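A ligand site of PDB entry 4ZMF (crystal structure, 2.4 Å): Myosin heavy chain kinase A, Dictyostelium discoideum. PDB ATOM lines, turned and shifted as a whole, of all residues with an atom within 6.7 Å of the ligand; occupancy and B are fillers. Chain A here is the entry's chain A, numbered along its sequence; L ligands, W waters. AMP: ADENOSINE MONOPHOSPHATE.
The backbone carbonyl oxygen (O) of Glu 179 sits at hydrogen-bond distance from the backbone NH (N) of Val 109, at 2.9 Å.
The backbone carbonyl oxygen of Ala 53 sits at hydrogen-bond distance from the backbone NH of Ala 60 (3.0 Å).
OE1 of Glu 179 sits at hydrogen-bond distance from OG1 of Thr 231 (2.6 Å).
The guanidinium group of Arg 58 is in hydrogen-bond range of OD2 of PHD 232.
The backbone carbonyl oxygen (O) of Ala 60 sits at hydrogen-bond distance from the backbone NH (N) of Phe 52 (2.9 Å).
N of Thr 231 is in hydrogen-bond range of O of Gln 224.
NZ of Lys 111 is in salt-bridge range of OE2 of Glu 179 (3.1 Å).
Phe 52 touches the ligand (CE1 to N3, 3.8 Å).
Ala 53 touches the ligand.
C of Glu 54 touches C5' of the ligand (3.9 Å).
Gly 55 touches the ligand (N to C5', 3.7 Å).
CB of Ala 60 touches O4' of the ligand (3.96 Å).
Val 109 touches the ligand.
Leu 155 touches the ligand.
Leu 181 touches the ligand (C to N1, 3.8 Å).
Phe 186 touches the ligand.
Thr 231 touches the ligand.
15 residues have an atom within 4 Å of the ligand: Phe 52, Ala 53, Glu 54, Gly 55, Arg 58, Ala 60, Val 109, Lys 111, Leu 155, Glu 179, Pro 180, Leu 181, Leu 182, Phe 186 and Thr 231.
The side-chain amino group (NZ) of Lys 111 is in salt-bridge range of an oxygen (O3P) of the ligand (3.1 Å).
NE of Arg 58 is in salt-bridge range of O2P of the ligand (3.2 Å).
The side-chain carboxylate (OE1) of Glu 179 is in hydrogen-bond range of a nitrogen (N6) of the ligand, at 2.8 Å.
The backbone carbonyl oxygen of Pro 180 lies within hydrogen-bond range of a nitrogen (N6) of the ligand (3.0 Å).
N of Leu 182 is in hydrogen-bond range of N1 of the ligand, 2.9 Å away.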
ATOM      1  N   PHE A  52      28.462  -7.795  -1.284  1.00  0.00           N
ATOM      2  CA  PHE A  52      28.775  -8.002   0.119  1.00  0.00           C
ATOM      3  C   PHE A  52      30.004  -8.875   0.303  1.00  0.00           C
ATOM      4  O   PHE A  52      30.441  -9.104   1.430  1.00  0.00           O
ATOM      5  CB  PHE A  52      27.610  -8.631   0.873  1.00  0.00           C
ATOM      6  CG  PHE A  52      27.314 -10.061   0.479  1.00  0.00           C
ATOM      7  CD1 PHE A  52      27.955 -11.145   1.118  1.00  0.00           C
ATOM      8  CD2 PHE A  52      26.407 -10.330  -0.510  1.00  0.00           C
ATOM      9  CE1 PHE A  52      27.668 -12.443   0.740  1.00  0.00           C
ATOM     10  CE2 PHE A  52      26.118 -11.629  -0.878  1.00  0.00           C
ATOM     11  CZ  PHE A  52      26.750 -12.685  -0.258  1.00  0.00           C
ATOM     12  N   ALA A  53      30.554  -9.391  -0.785  1.00  0.00           N
ATOM     13  CA  ALA A  53      31.786 -10.149  -0.720  1.00  0.00           C
ATOM     14  C   ALA A  53      32.409 -10.287  -2.100  1.00  0.00           C
ATOM     15  O   ALA A  53      31.755 -10.087  -3.119  1.00  0.00           O
ATOM     16  CB  ALA A  53      31.541 -11.515  -0.103  1.00  0.00           C
ATOM     17  N   GLU A  54      33.698 -10.592  -2.126  1.00  0.00           N
ATOM     18  CA  GLU A  54      34.360 -10.935  -3.368  1.00  0.00           C
ATOM     19  C   GLU A  54      35.374 -12.049  -3.130  1.00  0.00           C
ATOM     20  O   GLU A  54      35.962 -12.158  -2.041  1.00  0.00           O
ATOM     21  CB  GLU A  54      35.009  -9.716  -4.014  1.00  0.00           C
ATOM     22  CG  GLU A  54      36.283  -9.219  -3.327  1.00  0.00           C
ATOM     23  CD  GLU A  54      37.070  -8.222  -4.156  1.00  0.00           C
ATOM     24  OE1 GLU A  54      36.945  -8.212  -5.410  1.00  0.00           O
ATOM     25  OE2 GLU A  54      37.843  -7.445  -3.557  1.00  0.00           O
ATOM     26  N   GLY A  55      35.544 -12.877  -4.144  1.00  0.00           N
ATOM     27  CA  GLY A  55      36.638 -13.843  -4.232  1.00  0.00           C
ATOM     28  C   GLY A  55      37.591 -13.371  -5.303  1.00  0.00           C
ATOM     29  O   GLY A  55      37.581 -12.182  -5.683  1.00  0.00           O
ATOM     30  N   ALA A  56      38.408 -14.287  -5.820  1.00  0.00           N
ATOM     31  CA  ALA A  56      39.440 -13.958  -6.810  1.00  0.00           C
ATOM     32  C   ALA A  56      38.856 -13.429  -8.137  1.00  0.00           C
ATOM     33  O   ALA A  56      39.414 -12.499  -8.732  1.00  0.00           O
ATOM     34  CB  ALA A  56      40.324 -15.160  -7.069  1.00  0.00           C
ATOM     35  N   LEU A  57      37.727 -14.004  -8.558  1.00  0.00           N
ATOM     36  CA  LEU A  57      37.147 -13.729  -9.893  1.00  0.00           C
ATOM     37  C   LEU A  57      35.737 -13.105  -9.916  1.00  0.00           C
ATOM     38  O   LEU A  57      35.365 -12.445 -10.899  1.00  0.00           O
ATOM     39  CB  LEU A  57      37.113 -15.027 -10.713  1.00  0.00           C
ATOM     40  CG  LEU A  57      38.445 -15.795 -10.824  1.00  0.00           C
ATOM     41  CD1 LEU A  57      38.201 -17.156 -11.468  1.00  0.00           C
ATOM     42  CD2 LEU A  57      39.489 -14.990 -11.594  1.00  0.00           C
ATOM     43  N   ARG A  58      34.956 -13.278  -8.848  1.00  0.00           N
ATOM     44  CA  ARG A  58      33.555 -12.882  -8.855  1.00  0.00           C
ATOM     45  C   ARG A  58      33.170 -12.033  -7.655  1.00  0.00           C
ATOM     46  O   ARG A  58      33.860 -12.030  -6.647  1.00  0.00           O
ATOM     47  CB  ARG A  58      32.664 -14.110  -8.841  1.00  0.00           C
ATOM     48  CG  ARG A  58      32.977 -15.102  -9.948  1.00  0.00           C
ATOM     49  CD  ARG A  58      31.957 -16.214 -10.019  1.00  0.00           C
ATOM     50  NE  ARG A  58      32.114 -17.148  -8.915  1.00  0.00           N
ATOM     51  CZ  ARG A  58      31.447 -18.292  -8.796  1.00  0.00           C
ATOM     52  NH1 ARG A  58      30.563 -18.653  -9.719  1.00  0.00           N
ATOM     53  NH2 ARG A  58      31.670 -19.087  -7.755  1.00  0.00           N
ATOM     54  N   GLU A  59      32.048 -11.352  -7.768  1.00  0.00           N
ATOM     55  CA  GLU A  59      31.463 -10.655  -6.625  1.00  0.00           C
ATOM     56  C   GLU A  59      30.100 -11.256  -6.306  1.00  0.00           C
ATOM     57  O   GLU A  59      29.379 -11.660  -7.202  1.00  0.00           O
ATOM     58  CB  GLU A  59      31.339  -9.159  -6.932  1.00  0.00           C
ATOM     59  CG  GLU A  59      32.674  -8.431  -7.078  1.00  0.00           C
ATOM     60  CD  GLU A  59      32.577  -7.093  -7.807  1.00  0.00           C
ATOM     61  OE1 GLU A  59      31.571  -6.833  -8.499  1.00  0.00           O
ATOM     62  OE2 GLU A  59      33.512  -6.282  -7.684  1.00  0.00           O
ATOM     63  N   ALA A  60      29.753 -11.299  -5.026  1.00  0.00           N
ATOM     64  CA  ALA A  60      28.479 -11.798  -4.595  1.00  0.00           C
ATOM     65  C   ALA A  60      27.576 -10.680  -4.124  1.00  0.00           C
ATOM     66  O   ALA A  60      28.012  -9.818  -3.376  1.00  0.00           O
ATOM     67  CB  ALA A  60      28.681 -12.773  -3.456  1.00  0.00           C
ATOM     68  N   HIS A  62      23.648  -9.647  -2.413  1.00  0.00           N
ATOM     69  CA  HIS A  62      22.343 -10.020  -1.862  1.00  0.00           C
ATOM     70  C   HIS A  62      21.255  -9.640  -2.864  1.00  0.00           C
ATOM     71  O   HIS A  62      21.348  -8.602  -3.528  1.00  0.00           O
ATOM     72  CB  HIS A  62      22.052  -9.347  -0.540  1.00  0.00           C
ATOM     73  CG  HIS A  62      22.940  -9.808   0.547  1.00  0.00           C
ATOM     74  ND1 HIS A  62      22.970 -11.115   0.958  1.00  0.00           N
ATOM     75  CD2 HIS A  62      23.855  -9.141   1.295  1.00  0.00           C
ATOM     76  CE1 HIS A  62      23.868 -11.242   1.931  1.00  0.00           C
ATOM     77  NE2 HIS A  62      24.421 -10.058   2.144  1.00  0.00           N
ATOM     78  N   VAL A 109      21.616 -15.264  -3.317  1.00  0.00           N
ATOM     79  CA  VAL A 109      22.888 -14.662  -3.726  1.00  0.00           C
ATOM     80  C   VAL A 109      23.065 -14.763  -5.231  1.00  0.00           C
ATOM     81  O   VAL A 109      22.738 -15.776  -5.841  1.00  0.00           O
ATOM     82  CB  VAL A 109      24.065 -15.368  -3.010  1.00  0.00           C
ATOM     83  CG1 VAL A 109      25.417 -14.907  -3.542  1.00  0.00           C
ATOM     84  CG2 VAL A 109      23.988 -15.119  -1.499  1.00  0.00           C
ATOM     85  N   LYS A 111      26.009 -14.063  -8.303  1.00  0.00           N
ATOM     86  CA  LYS A 111      27.434 -13.926  -8.489  1.00  0.00           C
ATOM     87  C   LYS A 111      27.745 -13.502  -9.897  1.00  0.00           C
ATOM     88  O   LYS A 111      27.293 -14.122 -10.856  1.00  0.00           O
ATOM     89  CB  LYS A 111      28.151 -15.254  -8.159  1.00  0.00           C
ATOM     90  CG  LYS A 111      28.073 -15.621  -6.688  1.00  0.00           C
ATOM     91  CD  LYS A 111      28.699 -16.988  -6.401  1.00  0.00           C
ATOM     92  CE  LYS A 111      28.465 -17.460  -4.973  1.00  0.00           C
ATOM     93  NZ  LYS A 111      29.243 -18.684  -4.609  1.00  0.00           N
ATOM     94  N   LEU A 112      28.518 -12.422 -10.012  1.00  0.00           N
ATOM     95  CA  LEU A 112      28.944 -11.874 -11.291  1.00  0.00           C
ATOM     96  C   LEU A 112      30.441 -11.924 -11.371  1.00  0.00           C
ATOM     97  O   LEU A 112      31.126 -11.629 -10.402  1.00  0.00           O
ATOM     98  CB  LEU A 112      28.560 -10.397 -11.405  1.00  0.00           C
ATOM     99  CG  LEU A 112      27.204  -9.908 -11.904  1.00  0.00           C
ATOM    100  CD1 LEU A 112      27.236  -8.388 -11.880  1.00  0.00           C
ATOM    101  CD2 LEU A 112      26.850 -10.408 -13.302  1.00  0.00           C
ATOM    102  N   LEU A 155      24.464 -26.874  -2.091  1.00  0.00           N
ATOM    103  CA  LEU A 155      23.396 -26.001  -2.552  1.00  0.00           C
ATOM    104  C   LEU A 155      23.101 -26.175  -4.045  1.00  0.00           C
ATOM    105  O   LEU A 155      23.997 -26.463  -4.844  1.00  0.00           O
ATOM    106  CB  LEU A 155      23.802 -24.543  -2.327  1.00  0.00           C
ATOM    107  CG  LEU A 155      23.956 -24.076  -0.880  1.00  0.00           C
ATOM    108  CD1 LEU A 155      24.378 -22.623  -0.898  1.00  0.00           C
ATOM    109  CD2 LEU A 155      22.687 -24.248  -0.083  1.00  0.00           C
ATOM    110  N   GLU A 179      22.339 -18.684  -6.259  1.00  0.00           N
ATOM    111  CA  GLU A 179      22.258 -19.814  -5.326  1.00  0.00           C
ATOM    112  C   GLU A 179      21.671 -19.304  -4.020  1.00  0.00           C
ATOM    113  O   GLU A 179      21.607 -18.101  -3.835  1.00  0.00           O
ATOM    114  CB  GLU A 179      23.652 -20.425  -5.110  1.00  0.00           C
ATOM    115  CG  GLU A 179      24.708 -19.433  -4.646  1.00  0.00           C
ATOM    116  CD  GLU A 179      26.124 -20.006  -4.688  1.00  0.00           C
ATOM    117  OE1 GLU A 179      26.671 -20.312  -3.609  1.00  0.00           O
ATOM    118  OE2 GLU A 179      26.701 -20.115  -5.786  1.00  0.00           O
ATOM    119  N   PRO A 180      21.198 -20.193  -3.137  1.00  0.00           N
ATOM    120  CA  PRO A 180      20.680 -19.782  -1.860  1.00  0.00           C
ATOM    121  C   PRO A 180      21.704 -19.107  -0.976  1.00  0.00           C
ATOM    122  O   PRO A 180      22.911 -19.237  -1.204  1.00  0.00           O
ATOM    123  CB  PRO A 180      20.254 -21.099  -1.211  1.00  0.00           C
ATOM    124  CG  PRO A 180      20.070 -22.049  -2.319  1.00  0.00           C
ATOM    125  CD  PRO A 180      21.121 -21.654  -3.298  1.00  0.00           C
ATOM    126  N   LEU A 181      21.207 -18.379   0.013  1.00  0.00           N
ATOM    127  CA  LEU A 181      22.066 -17.640   0.933  1.00  0.00           C
ATOM    128  C   LEU A 181      22.541 -18.599   1.995  1.00  0.00           C
ATOM    129  O   LEU A 181      21.730 -19.327   2.593  1.00  0.00           O
ATOM    130  CB  LEU A 181      21.300 -16.475   1.570  1.00  0.00           C
ATOM    131  CG  LEU A 181      22.032 -15.580   2.596  1.00  0.00           C
ATOM    132  CD1 LEU A 181      23.201 -14.799   2.002  1.00  0.00           C
ATOM    133  CD2 LEU A 181      21.034 -14.633   3.244  1.00  0.00           C
ATOM    134  N   LEU A 182      23.845 -18.634   2.218  1.00  0.00           N
ATOM    135  CA  LEU A 182      24.387 -19.334   3.384  1.00  0.00           C
ATOM    136  C   LEU A 182      24.441 -18.382   4.579  1.00  0.00           C
ATOM    137  O   LEU A 182      25.087 -17.345   4.506  1.00  0.00           O
ATOM    138  CB  LEU A 182      25.797 -19.844   3.112  1.00  0.00           C
ATOM    139  CG  LEU A 182      25.918 -21.001   2.133  1.00  0.00           C
ATOM    140  CD1 LEU A 182      27.361 -21.164   1.692  1.00  0.00           C
ATOM    141  CD2 LEU A 182      25.378 -22.259   2.755  1.00  0.00           C
ATOM    142  N   VAL A 183      23.810 -18.764   5.683  1.00  0.00           N
ATOM    143  CA  VAL A 183      23.857 -17.976   6.920  1.00  0.00           C
ATOM    144  C   VAL A 183      24.856 -18.578   7.890  1.00  0.00           C
ATOM    145  O   VAL A 183      24.695 -19.706   8.335  1.00  0.00           O
ATOM    146  CB  VAL A 183      22.468 -17.971   7.631  1.00  0.00           C
ATOM    147  CG1 VAL A 183      22.514 -17.135   8.904  1.00  0.00           C
ATOM    148  CG2 VAL A 183      21.413 -17.431   6.684  1.00  0.00           C
ATOM    149  N   PHE A 186      31.507 -18.646   6.744  1.00  0.00           N
ATOM    150  CA  PHE A 186      31.894 -19.357   5.539  1.00  0.00           C
ATOM    151  C   PHE A 186      33.351 -19.774   5.626  1.00  0.00           C
ATOM    152  O   PHE A 186      34.229 -18.929   5.710  1.00  0.00           O
ATOM    153  CB  PHE A 186      31.694 -18.436   4.343  1.00  0.00           C
ATOM    154  CG  PHE A 186      31.783 -19.120   3.001  1.00  0.00           C
ATOM    155  CD1 PHE A 186      33.029 -19.378   2.407  1.00  0.00           C
ATOM    156  CD2 PHE A 186      30.635 -19.438   2.287  1.00  0.00           C
ATOM    157  CE1 PHE A 186      33.107 -19.956   1.147  1.00  0.00           C
ATOM    158  CE2 PHE A 186      30.705 -20.005   1.037  1.00  0.00           C
ATOM    159  CZ  PHE A 186      31.943 -20.275   0.461  1.00  0.00           C
ATOM    160  N   GLN A 224      33.815 -26.090   0.418  1.00  0.00           N
ATOM    161  CA  GLN A 224      33.707 -24.843   1.163  1.00  0.00           C
ATOM    162  C   GLN A 224      32.270 -24.450   1.365  1.00  0.00           C
ATOM    163  O   GLN A 224      31.425 -24.744   0.539  1.00  0.00           O
ATOM    164  CB  GLN A 224      34.404 -23.718   0.423  1.00  0.00           C
ATOM    165  CG  GLN A 224      33.836 -23.469  -0.963  1.00  0.00           C
ATOM    166  CD  GLN A 224      34.743 -22.591  -1.792  1.00  0.00           C
ATOM    167  OE1 GLN A 224      35.378 -21.687  -1.267  1.00  0.00           O
ATOM    168  NE2 GLN A 224      34.846 -22.877  -3.076  1.00  0.00           N
ATOM    169  N   VAL A 226      29.320 -23.279   4.823  1.00  0.00           N
ATOM    170  CA  VAL A 226      29.032 -23.084   6.214  1.00  0.00           C
ATOM    171  C   VAL A 226      28.636 -24.394   6.828  1.00  0.00           C
ATOM    172  O   VAL A 226      27.614 -24.976   6.448  1.00  0.00           O
ATOM    173  CB  VAL A 226      27.872 -22.099   6.425  1.00  0.00           C
ATOM    174  CG1 VAL A 226      27.469 -22.021   7.902  1.00  0.00           C
ATOM    175  CG2 VAL A 226      28.273 -20.716   5.932  1.00  0.00           C
ATOM    176  N   THR A 231      29.175 -25.065  -1.203  1.00  0.00           N
ATOM    177  CA  THR A 231      28.947 -24.438  -2.489  1.00  0.00           C
ATOM    178  C   THR A 231      30.240 -24.198  -3.232  1.00  0.00           C
ATOM    179  O   THR A 231      31.292 -24.305  -2.647  1.00  0.00           O
ATOM    180  CB  THR A 231      28.136 -23.117  -2.315  1.00  0.00           C
ATOM    181  OG1 THR A 231      27.605 -22.721  -3.575  1.00  0.00           O
ATOM    182  CG2 THR A 231      29.000 -21.996  -1.720  1.00  0.00           C
ATOM    183  N   PHD A 232      30.136 -23.880  -4.530  1.00  0.00           N
ATOM    184  CA  PHD A 232      31.303 -23.737  -5.411  1.00  0.00           C
ATOM    185  C   PHD A 232      32.361 -24.828  -5.264  1.00  0.00           C
ATOM    186  O   PHD A 232      33.509 -24.538  -5.005  1.00  0.00           O
ATOM    187  CB  PHD A 232      31.969 -22.341  -5.275  1.00  0.00           C
ATOM    188  CG  PHD A 232      32.580 -22.023  -6.647  1.00  0.00           C
ATOM    189  OD1 PHD A 232      34.014 -21.984  -6.954  1.00  0.00           O
ATOM    190  OD2 PHD A 232      31.834 -21.823  -7.623  1.00  0.00           O
ATOM    191  P   PHD A 232      34.665 -23.021  -8.072  1.00  0.00           P
ATOM    192  OP1 PHD A 232      35.566 -22.203  -8.980  1.00  0.00           O
ATOM    193  OP2 PHD A 232      33.508 -23.679  -8.826  1.00  0.00           O
ATOM    194  OP3 PHD A 232      35.388 -23.945  -7.090  1.00  0.00           O
HETATM  195  P   AMP L   1      33.007 -16.870  -4.574  1.00  0.00           P
HETATM  196  O1P AMP L   1      34.410 -16.825  -3.943  1.00  0.00           O
HETATM  197  O2P AMP L   1      32.874 -16.217  -5.931  1.00  0.00           O
HETATM  198  O3P AMP L   1      32.308 -18.230  -4.497  1.00  0.00           O
HETATM  199  O5' AMP L   1      32.059 -15.907  -3.677  1.00  0.00           O
HETATM  200  C5' AMP L   1      32.552 -14.743  -2.997  1.00  0.00           C
HETATM  201  C4' AMP L   1      32.445 -14.910  -1.478  1.00  0.00           C
HETATM  202  O4' AMP L   1      31.079 -14.810  -1.049  1.00  0.00           O
HETATM  203  C3' AMP L   1      32.938 -16.230  -0.925  1.00  0.00           C
HETATM  204  O3' AMP L   1      34.344 -16.251  -0.712  1.00  0.00           O
HETATM  205  C2' AMP L   1      32.163 -16.306   0.369  1.00  0.00           C
HETATM  206  O2' AMP L   1      32.780 -15.536   1.399  1.00  0.00           O
HETATM  207  C1' AMP L   1      30.821 -15.683   0.052  1.00  0.00           C
HETATM  208  N9  AMP L   1      29.779 -16.619  -0.455  1.00  0.00           N
HETATM  209  C8  AMP L   1      29.912 -17.426  -1.525  1.00  0.00           C
HETATM  210  N7  AMP L   1      28.785 -18.121  -1.744  1.00  0.00           N
HETATM  211  C5  AMP L   1      27.913 -17.758  -0.808  1.00  0.00           C
HETATM  212  C6  AMP L   1      26.535 -18.111  -0.495  1.00  0.00           C
HETATM  213  N6  AMP L   1      25.928 -19.014  -1.260  1.00  0.00           N
HETATM  214  N1  AMP L   1      25.926 -17.538   0.548  1.00  0.00           N
HETATM  215  C2  AMP L   1      26.601 -16.630   1.296  1.00  0.00           C
HETATM  216  N3  AMP L   1      27.867 -16.257   1.055  1.00  0.00           N
HETATM  217  C4  AMP L   1      28.567 -16.766   0.038  1.00  0.00           C
HETATM  218  O   HOH W   1      28.910 -15.277   3.700  1.00  0.00           O
